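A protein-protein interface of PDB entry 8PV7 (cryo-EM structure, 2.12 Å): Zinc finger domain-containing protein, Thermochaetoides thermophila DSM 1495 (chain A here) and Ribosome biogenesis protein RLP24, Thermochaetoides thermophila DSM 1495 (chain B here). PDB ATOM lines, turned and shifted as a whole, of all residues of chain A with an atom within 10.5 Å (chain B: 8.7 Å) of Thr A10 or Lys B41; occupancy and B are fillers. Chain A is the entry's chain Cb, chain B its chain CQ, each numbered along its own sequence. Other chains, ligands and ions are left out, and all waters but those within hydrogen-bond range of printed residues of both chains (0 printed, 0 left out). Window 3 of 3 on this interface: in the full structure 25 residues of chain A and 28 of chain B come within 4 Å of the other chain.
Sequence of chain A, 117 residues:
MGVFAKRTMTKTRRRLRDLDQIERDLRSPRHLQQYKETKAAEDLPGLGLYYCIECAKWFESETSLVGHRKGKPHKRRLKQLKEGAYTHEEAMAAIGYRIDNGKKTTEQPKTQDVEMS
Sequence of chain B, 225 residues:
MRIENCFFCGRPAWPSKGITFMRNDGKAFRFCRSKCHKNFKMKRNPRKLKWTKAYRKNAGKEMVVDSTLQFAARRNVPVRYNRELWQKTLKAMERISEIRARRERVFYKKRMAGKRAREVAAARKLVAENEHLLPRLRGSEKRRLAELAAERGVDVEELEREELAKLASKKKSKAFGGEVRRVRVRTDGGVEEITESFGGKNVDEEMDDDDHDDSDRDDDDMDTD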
ATOM      1  N   VAL A   3       7.568  31.261   2.521  1.00  0.00           N
ATOM      2  CA  VAL A   3       7.051  30.293   1.562  1.00  0.00           C
ATOM      3  C   VAL A   3       7.433  30.758   0.166  1.00  0.00           C
ATOM      4  O   VAL A   3       7.178  31.910  -0.200  1.00  0.00           O
ATOM      5  CB  VAL A   3       5.526  30.132   1.688  1.00  0.00           C
ATOM      6  CG1 VAL A   3       5.028  29.024   0.772  1.00  0.00           C
ATOM      7  CG2 VAL A   3       5.134  29.864   3.129  1.00  0.00           C
ATOM      8  N   PHE A   4       8.047  29.866  -0.606  1.00  0.00           N
ATOM      9  CA  PHE A   4       8.408  30.185  -1.980  1.00  0.00           C
ATOM     10  C   PHE A   4       7.155  30.299  -2.837  1.00  0.00           C
ATOM     11  O   PHE A   4       6.352  29.364  -2.893  1.00  0.00           O
ATOM     12  CB  PHE A   4       9.335  29.111  -2.543  1.00  0.00           C
ATOM     13  CG  PHE A   4       9.425  29.111  -4.041  1.00  0.00           C
ATOM     14  CD1 PHE A   4      10.189  30.059  -4.696  1.00  0.00           C
ATOM     15  CD2 PHE A   4       8.754  28.158  -4.796  1.00  0.00           C
ATOM     16  CE1 PHE A   4      10.281  30.064  -6.072  1.00  0.00           C
ATOM     17  CE2 PHE A   4       8.835  28.164  -6.175  1.00  0.00           C
ATOM     18  CZ  PHE A   4       9.601  29.117  -6.811  1.00  0.00           C
ATOM     19  N   ALA A   5       7.010  31.444  -3.511  1.00  0.00           N
ATOM     20  CA  ALA A   5       5.909  31.733  -4.435  1.00  0.00           C
ATOM     21  C   ALA A   5       4.553  31.544  -3.754  1.00  0.00           C
ATOM     22  O   ALA A   5       3.755  30.679  -4.114  1.00  0.00           O
ATOM     23  CB  ALA A   5       6.022  30.891  -5.707  1.00  0.00           C
ATOM     24  N   LYS A   6       4.314  32.391  -2.749  1.00  0.00           N
ATOM     25  CA  LYS A   6       3.159  32.237  -1.867  1.00  0.00           C
ATOM     26  C   LYS A   6       1.841  32.484  -2.599  1.00  0.00           C
ATOM     27  O   LYS A   6       0.798  31.965  -2.184  1.00  0.00           O
ATOM     28  CB  LYS A   6       3.324  33.183  -0.669  1.00  0.00           C
ATOM     29  CG  LYS A   6       2.168  33.227   0.329  1.00  0.00           C
ATOM     30  CD  LYS A   6       2.626  33.361   1.779  1.00  0.00           C
ATOM     31  CE  LYS A   6       3.839  34.263   1.928  1.00  0.00           C
ATOM     32  NZ  LYS A   6       3.769  35.079   3.166  1.00  0.00           N
ATOM     33  N   ARG A   7       1.878  33.230  -3.707  1.00  0.00           N
ATOM     34  CA  ARG A   7       0.665  33.575  -4.446  1.00  0.00           C
ATOM     35  C   ARG A   7      -0.055  32.343  -4.988  1.00  0.00           C
ATOM     36  O   ARG A   7      -1.279  32.227  -4.867  1.00  0.00           O
ATOM     37  CB  ARG A   7       1.020  34.530  -5.587  1.00  0.00           C
ATOM     38  CG  ARG A   7      -0.088  34.744  -6.607  1.00  0.00           C
ATOM     39  CD  ARG A   7       0.466  35.202  -7.948  1.00  0.00           C
ATOM     40  NE  ARG A   7       1.163  36.474  -7.825  1.00  0.00           N
ATOM     41  CZ  ARG A   7       0.589  37.659  -7.975  1.00  0.00           C
ATOM     42  NH1 ARG A   7      -0.687  37.772  -8.296  1.00  0.00           N
ATOM     43  NH2 ARG A   7       1.314  38.758  -7.793  1.00  0.00           N
ATOM     44  N   THR A   8       0.685  31.400  -5.565  1.00  0.00           N
ATOM     45  CA  THR A   8       0.102  30.205  -6.156  1.00  0.00           C
ATOM     46  C   THR A   8       0.204  28.992  -5.243  1.00  0.00           C
ATOM     47  O   THR A   8       0.175  27.857  -5.727  1.00  0.00           O
ATOM     48  CB  THR A   8       0.762  29.903  -7.502  1.00  0.00           C
ATOM     49  OG1 THR A   8       2.183  30.018  -7.377  1.00  0.00           O
ATOM     50  CG2 THR A   8       0.268  30.858  -8.569  1.00  0.00           C
ATOM     51  N   MET A   9       0.298  29.212  -3.932  1.00  0.00           N
ATOM     52  CA  MET A   9       0.532  28.127  -2.985  1.00  0.00           C
ATOM     53  C   MET A   9      -0.646  27.168  -2.874  1.00  0.00           C
ATOM     54  O   MET A   9      -0.441  25.995  -2.551  1.00  0.00           O
ATOM     55  CB  MET A   9       0.853  28.708  -1.609  1.00  0.00           C
ATOM     56  CG  MET A   9       1.638  27.784  -0.707  1.00  0.00           C
ATOM     57  SD  MET A   9       1.150  27.925   1.020  1.00  0.00           S
ATOM     58  CE  MET A   9       1.257  29.693   1.267  1.00  0.00           C
ATOM     59  N   THR A  10      -1.865  27.631  -3.128  1.00  0.00           N
ATOM     60  CA  THR A  10      -3.048  26.793  -2.992  1.00  0.00           C
ATOM     61  C   THR A  10      -3.442  26.091  -4.284  1.00  0.00           C
ATOM     62  O   THR A  10      -4.464  25.400  -4.301  1.00  0.00           O
ATOM     63  CB  THR A  10      -4.230  27.619  -2.483  1.00  0.00           C
ATOM     64  OG1 THR A  10      -4.418  28.764  -3.322  1.00  0.00           O
ATOM     65  CG2 THR A  10      -3.975  28.074  -1.064  1.00  0.00           C
ATOM     66  N   LYS A  11      -2.666  26.248  -5.353  1.00  0.00           N
ATOM     67  CA  LYS A  11      -2.951  25.544  -6.595  1.00  0.00           C
ATOM     68  C   LYS A  11      -2.786  24.041  -6.403  1.00  0.00           C
ATOM     69  O   LYS A  11      -1.977  23.582  -5.593  1.00  0.00           O
ATOM     70  CB  LYS A  11      -2.021  26.028  -7.709  1.00  0.00           C
ATOM     71  CG  LYS A  11      -2.466  27.298  -8.408  1.00  0.00           C
ATOM     72  CD  LYS A  11      -1.549  27.624  -9.575  1.00  0.00           C
ATOM     73  CE  LYS A  11      -2.164  28.642 -10.520  1.00  0.00           C
ATOM     74  NZ  LYS A  11      -3.265  28.077 -11.331  1.00  0.00           N
ATOM     75  N   THR A  12      -3.584  23.277  -7.151  1.00  0.00           N
ATOM     76  CA  THR A  12      -3.501  21.821  -7.099  1.00  0.00           C
ATOM     77  C   THR A  12      -2.134  21.321  -7.549  1.00  0.00           C
ATOM     78  O   THR A  12      -1.616  20.344  -6.999  1.00  0.00           O
ATOM     79  CB  THR A  12      -4.617  21.213  -7.952  1.00  0.00           C
ATOM     80  OG1 THR A  12      -5.878  21.731  -7.520  1.00  0.00           O
ATOM     81  CG2 THR A  12      -4.644  19.702  -7.835  1.00  0.00           C
ATOM     82  N   ARG A  13      -1.510  22.001  -8.507  1.00  0.00           N
ATOM     83  CA  ARG A  13      -0.171  21.618  -8.936  1.00  0.00           C
ATOM     84  C   ARG A  13       0.907  21.960  -7.911  1.00  0.00           C
ATOM     85  O   ARG A  13       2.065  21.590  -8.122  1.00  0.00           O
ATOM     86  CB  ARG A  13       0.155  22.262 -10.283  1.00  0.00           C
ATOM     87  CG  ARG A  13       0.273  23.773 -10.282  1.00  0.00           C
ATOM     88  CD  ARG A  13       0.931  24.229 -11.566  1.00  0.00           C
ATOM     89  NE  ARG A  13       0.795  25.660 -11.790  1.00  0.00           N
ATOM     90  CZ  ARG A  13       1.644  26.577 -11.347  1.00  0.00           C
ATOM     91  NH1 ARG A  13       2.693  26.252 -10.612  1.00  0.00           N
ATOM     92  NH2 ARG A  13       1.431  27.853 -11.647  1.00  0.00           N
ATOM     93  N   ARG A  14       0.567  22.654  -6.823  1.00  0.00           N
ATOM     94  CA  ARG A  14       1.479  22.901  -5.714  1.00  0.00           C
ATOM     95  C   ARG A  14       1.092  22.131  -4.456  1.00  0.00           C
ATOM     96  O   ARG A  14       1.558  22.473  -3.366  1.00  0.00           O
ATOM     97  CB  ARG A  14       1.540  24.398  -5.404  1.00  0.00           C
ATOM     98  CG  ARG A  14       2.065  25.259  -6.538  1.00  0.00           C
ATOM     99  CD  ARG A  14       3.567  25.429  -6.458  1.00  0.00           C
ATOM    100  NE  ARG A  14       4.001  25.916  -5.155  1.00  0.00           N
ATOM    101  CZ  ARG A  14       4.070  27.194  -4.813  1.00  0.00           C
ATOM    102  NH1 ARG A  14       3.738  28.155  -5.656  1.00  0.00           N
ATOM    103  NH2 ARG A  14       4.483  27.516  -3.592  1.00  0.00           N
ATOM    104  N   ARG A  15       0.259  21.100  -4.581  1.00  0.00           N
ATOM    105  CA  ARG A  15      -0.273  20.394  -3.421  1.00  0.00           C
ATOM    106  C   ARG A  15       0.804  19.545  -2.748  1.00  0.00           C
ATOM    107  O   ARG A  15       1.699  19.002  -3.399  1.00  0.00           O
ATOM    108  CB  ARG A  15      -1.454  19.519  -3.847  1.00  0.00           C
ATOM    109  CG  ARG A  15      -2.226  18.864  -2.720  1.00  0.00           C
ATOM    110  CD  ARG A  15      -3.147  17.777  -3.233  1.00  0.00           C
ATOM    111  NE  ARG A  15      -3.630  16.937  -2.146  1.00  0.00           N
ATOM    112  CZ  ARG A  15      -2.989  15.875  -1.679  1.00  0.00           C
ATOM    113  NH1 ARG A  15      -1.849  15.469  -2.210  1.00  0.00           N
ATOM    114  NH2 ARG A  15      -3.507  15.200  -0.659  1.00  0.00           N
ATOM    115  N   LEU A  16       0.709  19.438  -1.423  1.00  0.00           N
ATOM    116  CA  LEU A  16       1.608  18.633  -0.611  1.00  0.00           C
ATOM    117  C   LEU A  16       0.862  17.440  -0.025  1.00  0.00           C
ATOM    118  O   LEU A  16      -0.369  17.386  -0.035  1.00  0.00           O
ATOM    119  CB  LEU A  16       2.228  19.468   0.516  1.00  0.00           C
ATOM    120  CG  LEU A  16       2.875  20.783   0.077  1.00  0.00           C
ATOM    121  CD1 LEU A  16       3.431  21.531   1.269  1.00  0.00           C
ATOM    122  CD2 LEU A  16       3.955  20.543  -0.964  1.00  0.00           C
ATOM    123  N   ARG A  17       1.629  16.485   0.499  1.00  0.00           N
ATOM    124  CA  ARG A  17       1.060  15.258   1.044  1.00  0.00           C
ATOM    125  C   ARG A  17       0.282  15.534   2.328  1.00  0.00           C
ATOM    126  O   ARG A  17       0.680  16.359   3.152  1.00  0.00           O
ATOM    127  CB  ARG A  17       2.176  14.244   1.304  1.00  0.00           C
ATOM    128  CG  ARG A  17       1.708  12.839   1.635  1.00  0.00           C
ATOM    129  CD  ARG A  17       2.789  11.817   1.336  1.00  0.00           C
ATOM    130  NE  ARG A  17       2.385  10.456   1.666  1.00  0.00           N
ATOM    131  CZ  ARG A  17       1.639   9.681   0.891  1.00  0.00           C
ATOM    132  NH1 ARG A  17       1.186  10.101  -0.277  1.00  0.00           N
ATOM    133  NH2 ARG A  17       1.341   8.453   1.300  1.00  0.00           N
ATOM    134  N   ASP A  18      -0.834  14.832   2.494  1.00  0.00           N
ATOM    135  CA  ASP A  18      -1.751  15.098   3.594  1.00  0.00           C
ATOM    136  C   ASP A  18      -1.347  14.360   4.867  1.00  0.00           C
ATOM    137  O   ASP A  18      -0.627  13.354   4.837  1.00  0.00           O
ATOM    138  CB  ASP A  18      -3.175  14.704   3.205  1.00  0.00           C
ATOM    139  CG  ASP A  18      -4.027  15.897   2.836  1.00  0.00           C
ATOM    140  OD1 ASP A  18      -4.102  16.848   3.642  1.00  0.00           O
ATOM    141  OD2 ASP A  18      -4.629  15.883   1.742  1.00  0.00           O
ATOM    142  N   ARG A  77       4.833  19.345  12.947  1.00  0.00           N
ATOM    143  CA  ARG A  77       4.324  18.101  12.376  1.00  0.00           C
ATOM    144  C   ARG A  77       4.208  17.010  13.433  1.00  0.00           C
ATOM    145  O   ARG A  77       3.237  16.246  13.439  1.00  0.00           O
ATOM    146  CB  ARG A  77       5.211  17.644  11.221  1.00  0.00           C
ATOM    147  CG  ARG A  77       4.780  18.198   9.885  1.00  0.00           C
ATOM    148  CD  ARG A  77       3.423  17.651   9.480  1.00  0.00           C
ATOM    149  NE  ARG A  77       2.827  18.429   8.403  1.00  0.00           N
ATOM    150  CZ  ARG A  77       3.069  18.235   7.116  1.00  0.00           C
ATOM    151  NH1 ARG A  77       3.865  17.267   6.700  1.00  0.00           N
ATOM    152  NH2 ARG A  77       2.497  19.035   6.222  1.00  0.00           N
ATOM    153  N   PHE B   8     -15.691  18.316   6.017  1.00  0.00           N
ATOM    154  CA  PHE B   8     -15.012  19.289   6.861  1.00  0.00           C
ATOM    155  C   PHE B   8     -15.886  19.746   8.024  1.00  0.00           C
ATOM    156  O   PHE B   8     -15.447  19.729   9.176  1.00  0.00           O
ATOM    157  CB  PHE B   8     -14.568  20.481   6.018  1.00  0.00           C
ATOM    158  CG  PHE B   8     -13.414  21.235   6.601  1.00  0.00           C
ATOM    159  CD1 PHE B   8     -13.628  22.249   7.517  1.00  0.00           C
ATOM    160  CD2 PHE B   8     -12.117  20.931   6.231  1.00  0.00           C
ATOM    161  CE1 PHE B   8     -12.570  22.941   8.054  1.00  0.00           C
ATOM    162  CE2 PHE B   8     -11.056  21.625   6.762  1.00  0.00           C
ATOM    163  CZ  PHE B   8     -11.282  22.628   7.677  1.00  0.00           C
ATOM    164  N   ILE B  19     -18.328  20.565  -3.646  1.00  0.00           N
ATOM    165  CA  ILE B  19     -17.362  20.012  -4.586  1.00  0.00           C
ATOM    166  C   ILE B  19     -16.694  18.796  -3.956  1.00  0.00           C
ATOM    167  O   ILE B  19     -16.561  18.697  -2.735  1.00  0.00           O
ATOM    168  CB  ILE B  19     -16.342  21.101  -5.019  1.00  0.00           C
ATOM    169  CG1 ILE B  19     -15.575  20.686  -6.277  1.00  0.00           C
ATOM    170  CG2 ILE B  19     -15.403  21.488  -3.882  1.00  0.00           C
ATOM    171  CD1 ILE B  19     -14.735  21.783  -6.862  1.00  0.00           C
ATOM    172  N   PHE B  21     -13.292  16.320  -3.888  1.00  0.00           N
ATOM    173  CA  PHE B  21     -11.883  16.134  -4.182  1.00  0.00           C
ATOM    174  C   PHE B  21     -11.585  14.640  -4.248  1.00  0.00           C
ATOM    175  O   PHE B  21     -11.878  13.900  -3.307  1.00  0.00           O
ATOM    176  CB  PHE B  21     -11.029  16.830  -3.119  1.00  0.00           C
ATOM    177  CG  PHE B  21      -9.572  16.503  -3.191  1.00  0.00           C
ATOM    178  CD1 PHE B  21      -8.868  16.669  -4.367  1.00  0.00           C
ATOM    179  CD2 PHE B  21      -8.891  16.067  -2.067  1.00  0.00           C
ATOM    180  CE1 PHE B  21      -7.525  16.380  -4.432  1.00  0.00           C
ATOM    181  CE2 PHE B  21      -7.546  15.781  -2.125  1.00  0.00           C
ATOM    182  CZ  PHE B  21      -6.860  15.937  -3.310  1.00  0.00           C
ATOM    183  N   PHE B  31     -17.247  18.241   0.032  1.00  0.00           N
ATOM    184  CA  PHE B  31     -17.394  19.499   0.742  1.00  0.00           C
ATOM    185  C   PHE B  31     -18.700  20.157   0.341  1.00  0.00           C
ATOM    186  O   PHE B  31     -19.078  20.155  -0.833  1.00  0.00           O
ATOM    187  CB  PHE B  31     -16.227  20.445   0.452  1.00  0.00           C
ATOM    188  CG  PHE B  31     -14.895  19.828   0.695  1.00  0.00           C
ATOM    189  CD1 PHE B  31     -14.410  19.701   1.980  1.00  0.00           C
ATOM    190  CD2 PHE B  31     -14.138  19.346  -0.356  1.00  0.00           C
ATOM    191  CE1 PHE B  31     -13.196  19.116   2.210  1.00  0.00           C
ATOM    192  CE2 PHE B  31     -12.924  18.760  -0.127  1.00  0.00           C
ATOM    193  CZ  PHE B  31     -12.456  18.642   1.155  1.00  0.00           C
ATOM    194  N   ARG B  33     -19.330  23.394   0.600  1.00  0.00           N
ATOM    195  CA  ARG B  33     -19.168  24.760   0.117  1.00  0.00           C
ATOM    196  C   ARG B  33     -17.690  25.067  -0.090  1.00  0.00           C
ATOM    197  O   ARG B  33     -16.799  24.329   0.351  1.00  0.00           O
ATOM    198  CB  ARG B  33     -19.788  25.778   1.078  1.00  0.00           C
ATOM    199  CG  ARG B  33     -19.125  25.801   2.432  1.00  0.00           C
ATOM    200  CD  ARG B  33     -19.956  26.520   3.467  1.00  0.00           C
ATOM    201  NE  ARG B  33     -19.798  25.891   4.769  1.00  0.00           N
ATOM    202  CZ  ARG B  33     -20.371  26.312   5.886  1.00  0.00           C
ATOM    203  NH1 ARG B  33     -21.137  27.390   5.905  1.00  0.00           N
ATOM    204  NH2 ARG B  33     -20.171  25.636   7.011  1.00  0.00           N
ATOM    205  N   SER B  34     -17.449  26.201  -0.752  1.00  0.00           N
ATOM    206  CA  SER B  34     -16.086  26.622  -1.045  1.00  0.00           C
ATOM    207  C   SER B  34     -15.342  27.039   0.217  1.00  0.00           C
ATOM    208  O   SER B  34     -14.115  26.974   0.253  1.00  0.00           O
ATOM    209  CB  SER B  34     -16.088  27.754  -2.073  1.00  0.00           C
ATOM    210  OG  SER B  34     -16.952  28.806  -1.694  1.00  0.00           O
ATOM    211  N   LYS B  35     -16.064  27.455   1.261  1.00  0.00           N
ATOM    212  CA  LYS B  35     -15.428  27.785   2.536  1.00  0.00           C
ATOM    213  C   LYS B  35     -14.704  26.576   3.119  1.00  0.00           C
ATOM    214  O   LYS B  35     -13.501  26.630   3.419  1.00  0.00           O
ATOM    215  CB  LYS B  35     -16.487  28.306   3.508  1.00  0.00           C
ATOM    216  CG  LYS B  35     -16.033  28.478   4.948  1.00  0.00           C
ATOM    217  CD  LYS B  35     -17.231  28.715   5.850  1.00  0.00           C
ATOM    218  CE  LYS B  35     -16.839  29.187   7.237  1.00  0.00           C
ATOM    219  NZ  LYS B  35     -18.042  29.517   8.040  1.00  0.00           N
ATOM    220  N   CYS B  36     -15.422  25.456   3.230  1.00  0.00           N
ATOM    221  CA  CYS B  36     -14.830  24.210   3.703  1.00  0.00           C
ATOM    222  C   CYS B  36     -13.766  23.702   2.743  1.00  0.00           C
ATOM    223  O   CYS B  36     -12.715  23.217   3.180  1.00  0.00           O
ATOM    224  CB  CYS B  36     -15.922  23.162   3.889  1.00  0.00           C
ATOM    225  SG  CYS B  36     -17.304  23.725   4.880  1.00  0.00           S
ATOM    226  N   HIS B  37     -14.012  23.828   1.434  1.00  0.00           N
ATOM    227  CA  HIS B  37     -13.034  23.382   0.444  1.00  0.00           C
ATOM    228  C   HIS B  37     -11.714  24.142   0.562  1.00  0.00           C
ATOM    229  O   HIS B  37     -10.634  23.540   0.532  1.00  0.00           O
ATOM    230  CB  HIS B  37     -13.621  23.545  -0.954  1.00  0.00           C
ATOM    231  CG  HIS B  37     -12.749  23.018  -2.044  1.00  0.00           C
ATOM    232  ND1 HIS B  37     -12.576  23.677  -3.240  1.00  0.00           N
ATOM    233  CD2 HIS B  37     -12.013  21.885  -2.129  1.00  0.00           C
ATOM    234  CE1 HIS B  37     -11.767  22.978  -4.012  1.00  0.00           C
ATOM    235  NE2 HIS B  37     -11.408  21.888  -3.360  1.00  0.00           N
ATOM    236  N   LYS B  38     -11.780  25.462   0.734  1.00  0.00           N
ATOM    237  CA  LYS B  38     -10.570  26.270   0.796  1.00  0.00           C
ATOM    238  C   LYS B  38      -9.841  26.081   2.118  1.00  0.00           C
ATOM    239  O   LYS B  38      -8.607  26.102   2.152  1.00  0.00           O
ATOM    240  CB  LYS B  38     -10.911  27.739   0.558  1.00  0.00           C
ATOM    241  CG  LYS B  38     -11.284  28.047  -0.880  1.00  0.00           C
ATOM    242  CD  LYS B  38     -11.790  29.465  -1.044  1.00  0.00           C
ATOM    243  CE  LYS B  38     -12.217  29.725  -2.477  1.00  0.00           C
ATOM    244  NZ  LYS B  38     -12.580  31.144  -2.710  1.00  0.00           N
ATOM    245  N   ASN B  39     -10.578  25.869   3.212  1.00  0.00           N
ATOM    246  CA  ASN B  39      -9.915  25.541   4.472  1.00  0.00           C
ATOM    247  C   ASN B  39      -9.198  24.192   4.388  1.00  0.00           C
ATOM    248  O   ASN B  39      -8.077  24.037   4.898  1.00  0.00           O
ATOM    249  CB  ASN B  39     -10.931  25.566   5.612  1.00  0.00           C
ATOM    250  CG  ASN B  39     -11.233  26.976   6.084  1.00  0.00           C
ATOM    251  OD1 ASN B  39     -10.335  27.720   6.461  1.00  0.00           O
ATOM    252  ND2 ASN B  39     -12.498  27.350   6.057  1.00  0.00           N
ATOM    253  N   PHE B  40      -9.815  23.217   3.714  1.00  0.00           N
ATOM    254  CA  PHE B  40      -9.158  21.933   3.484  1.00  0.00           C
ATOM    255  C   PHE B  40      -7.897  22.089   2.636  1.00  0.00           C
ATOM    256  O   PHE B  40      -6.862  21.490   2.947  1.00  0.00           O
ATOM    257  CB  PHE B  40     -10.141  20.973   2.819  1.00  0.00           C
ATOM    258  CG  PHE B  40      -9.572  19.616   2.515  1.00  0.00           C
ATOM    259  CD1 PHE B  40      -9.578  18.623   3.474  1.00  0.00           C
ATOM    260  CD2 PHE B  40      -9.070  19.323   1.255  1.00  0.00           C
ATOM    261  CE1 PHE B  40      -9.072  17.376   3.196  1.00  0.00           C
ATOM    262  CE2 PHE B  40      -8.560  18.079   0.975  1.00  0.00           C
ATOM    263  CZ  PHE B  40      -8.563  17.103   1.945  1.00  0.00           C
ATOM    264  N   LYS B  41      -7.968  22.875   1.558  1.00  0.00           N
ATOM    265  CA  LYS B  41      -6.802  23.096   0.707  1.00  0.00           C
ATOM    266  C   LYS B  41      -5.712  23.885   1.415  1.00  0.00           C
ATOM    267  O   LYS B  41      -4.541  23.780   1.039  1.00  0.00           O
ATOM    268  CB  LYS B  41      -7.199  23.819  -0.578  1.00  0.00           C
ATOM    269  CG  LYS B  41      -8.062  23.005  -1.509  1.00  0.00           C
ATOM    270  CD  LYS B  41      -8.720  23.881  -2.553  1.00  0.00           C
ATOM    271  CE  LYS B  41      -7.702  24.534  -3.461  1.00  0.00           C
ATOM    272  NZ  LYS B  41      -7.012  23.533  -4.316  1.00  0.00           N
ATOM    273  N   MET B  42      -6.072  24.679   2.415  1.00  0.00           N
ATOM    274  CA  MET B  42      -5.103  25.326   3.281  1.00  0.00           C
ATOM    275  C   MET B  42      -4.643  24.430   4.416  1.00  0.00           C
ATOM    276  O   MET B  42      -3.821  24.868   5.222  1.00  0.00           O
ATOM    277  CB  MET B  42      -5.695  26.605   3.857  1.00  0.00           C
ATOM    278  CG  MET B  42      -5.880  27.699   2.847  1.00  0.00           C
ATOM    279  SD  MET B  42      -5.904  29.305   3.631  1.00  0.00           S
ATOM    280  CE  MET B  42      -7.668  29.431   3.844  1.00  0.00           C
ATOM    281  N   LYS B  43      -5.186  23.211   4.512  1.00  0.00           N
ATOM    282  CA  LYS B  43      -4.759  22.193   5.483  1.00  0.00           C
ATOM    283  C   LYS B  43      -5.069  22.631   6.912  1.00  0.00           C
ATOM    284  O   LYS B  43      -4.298  22.373   7.834  1.00  0.00           O
ATOM    285  CB  LYS B  43      -3.273  21.823   5.353  1.00  0.00           C
ATOM    286  CG  LYS B  43      -2.751  21.582   3.944  1.00  0.00           C
ATOM    287  CD  LYS B  43      -3.122  20.219   3.410  1.00  0.00           C
ATOM    288  CE  LYS B  43      -2.373  19.939   2.116  1.00  0.00           C
ATOM    289  NZ  LYS B  43      -2.529  18.541   1.650  1.00  0.00           N
ATOM    290  N   ARG B  44      -6.195  23.307   7.092  1.00  0.00           N
ATOM    291  CA  ARG B  44      -6.686  23.605   8.427  1.00  0.00           C
ATOM    292  C   ARG B  44      -7.369  22.375   9.011  1.00  0.00           C
ATOM    293  O   ARG B  44      -8.081  21.653   8.311  1.00  0.00           O
ATOM    294  CB  ARG B  44      -7.651  24.787   8.383  1.00  0.00           C
ATOM    295  CG  ARG B  44      -7.066  26.034   7.740  1.00  0.00           C
ATOM    296  CD  ARG B  44      -7.460  27.291   8.488  1.00  0.00           C
ATOM    297  NE  ARG B  44      -6.760  27.421   9.758  1.00  0.00           N
ATOM    298  CZ  ARG B  44      -6.991  28.378  10.644  1.00  0.00           C
ATOM    299  NH1 ARG B  44      -7.906  29.308  10.433  1.00  0.00           N
ATOM    300  NH2 ARG B  44      -6.286  28.403  11.769  1.00  0.00           N
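O of Thr A10 lies within hydrogen-bond range of NZ of Lys B41 (3.2 Å). The backbone carbonyl oxygen of Leu A16 sits at hydrogen-bond distance from the side-chain amino group of Lys B43 (3.0 Å). OD1 of Asp A18 is in salt-bridge range of NZ of Lys B43, at 3.1 Å.
OD2 of Asp A18 is in salt-bridge range of NH2 of Arg A15 (2.7 Å).
Printed residues of chain B within 4 Å of Thr A10: Lys B41 (3.2 Å). Of chain A, only Thr A10 (3.2 Å) and Thr A12 (3.8 Å) come within 4 Å of Lys B41. Of the printed residues of chain B, Thr A12 touches Lys B41 (3.8 Å). Printed residues of chain A within 4 Å of Phe B21: Arg A15. Printed residues of chain B within 4 Å of Leu A16: Lys B43. Printed residues of chain B within 4 Å of Arg A15: Phe B21 (3.6 Å). Met A9 touches none of the printed residues of chain B. Arg B44 touches none of the printed residues of chain A. The nearest printed residue of chain A that does not touch Lys B43 is Arg A17 (4.2 Å).
OG1 of Thr A12 touches NZ of Lys B41, 3.8 Å away. Phe B21 touches Arg A15 (CZ to NE, 3.6 Å).
Hydrophobic or aromatic side chains of chain B within 4 Å of the printed part of chain A: Phe B21. Of the 17 printed residues of chain A, 5 touch a printed residue of chain B. Printed residues of chain A that touch a printed residue of chain B: Thr A10, Thr A12, Arg A15, Leu A16 and Asp A18. Among the printed residues, Asp or Glu carboxylates within 4 Å of a Lys or Arg side-chain nitrogen of the other chain: Asp A18 with Lys B43 (3.1 Å).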
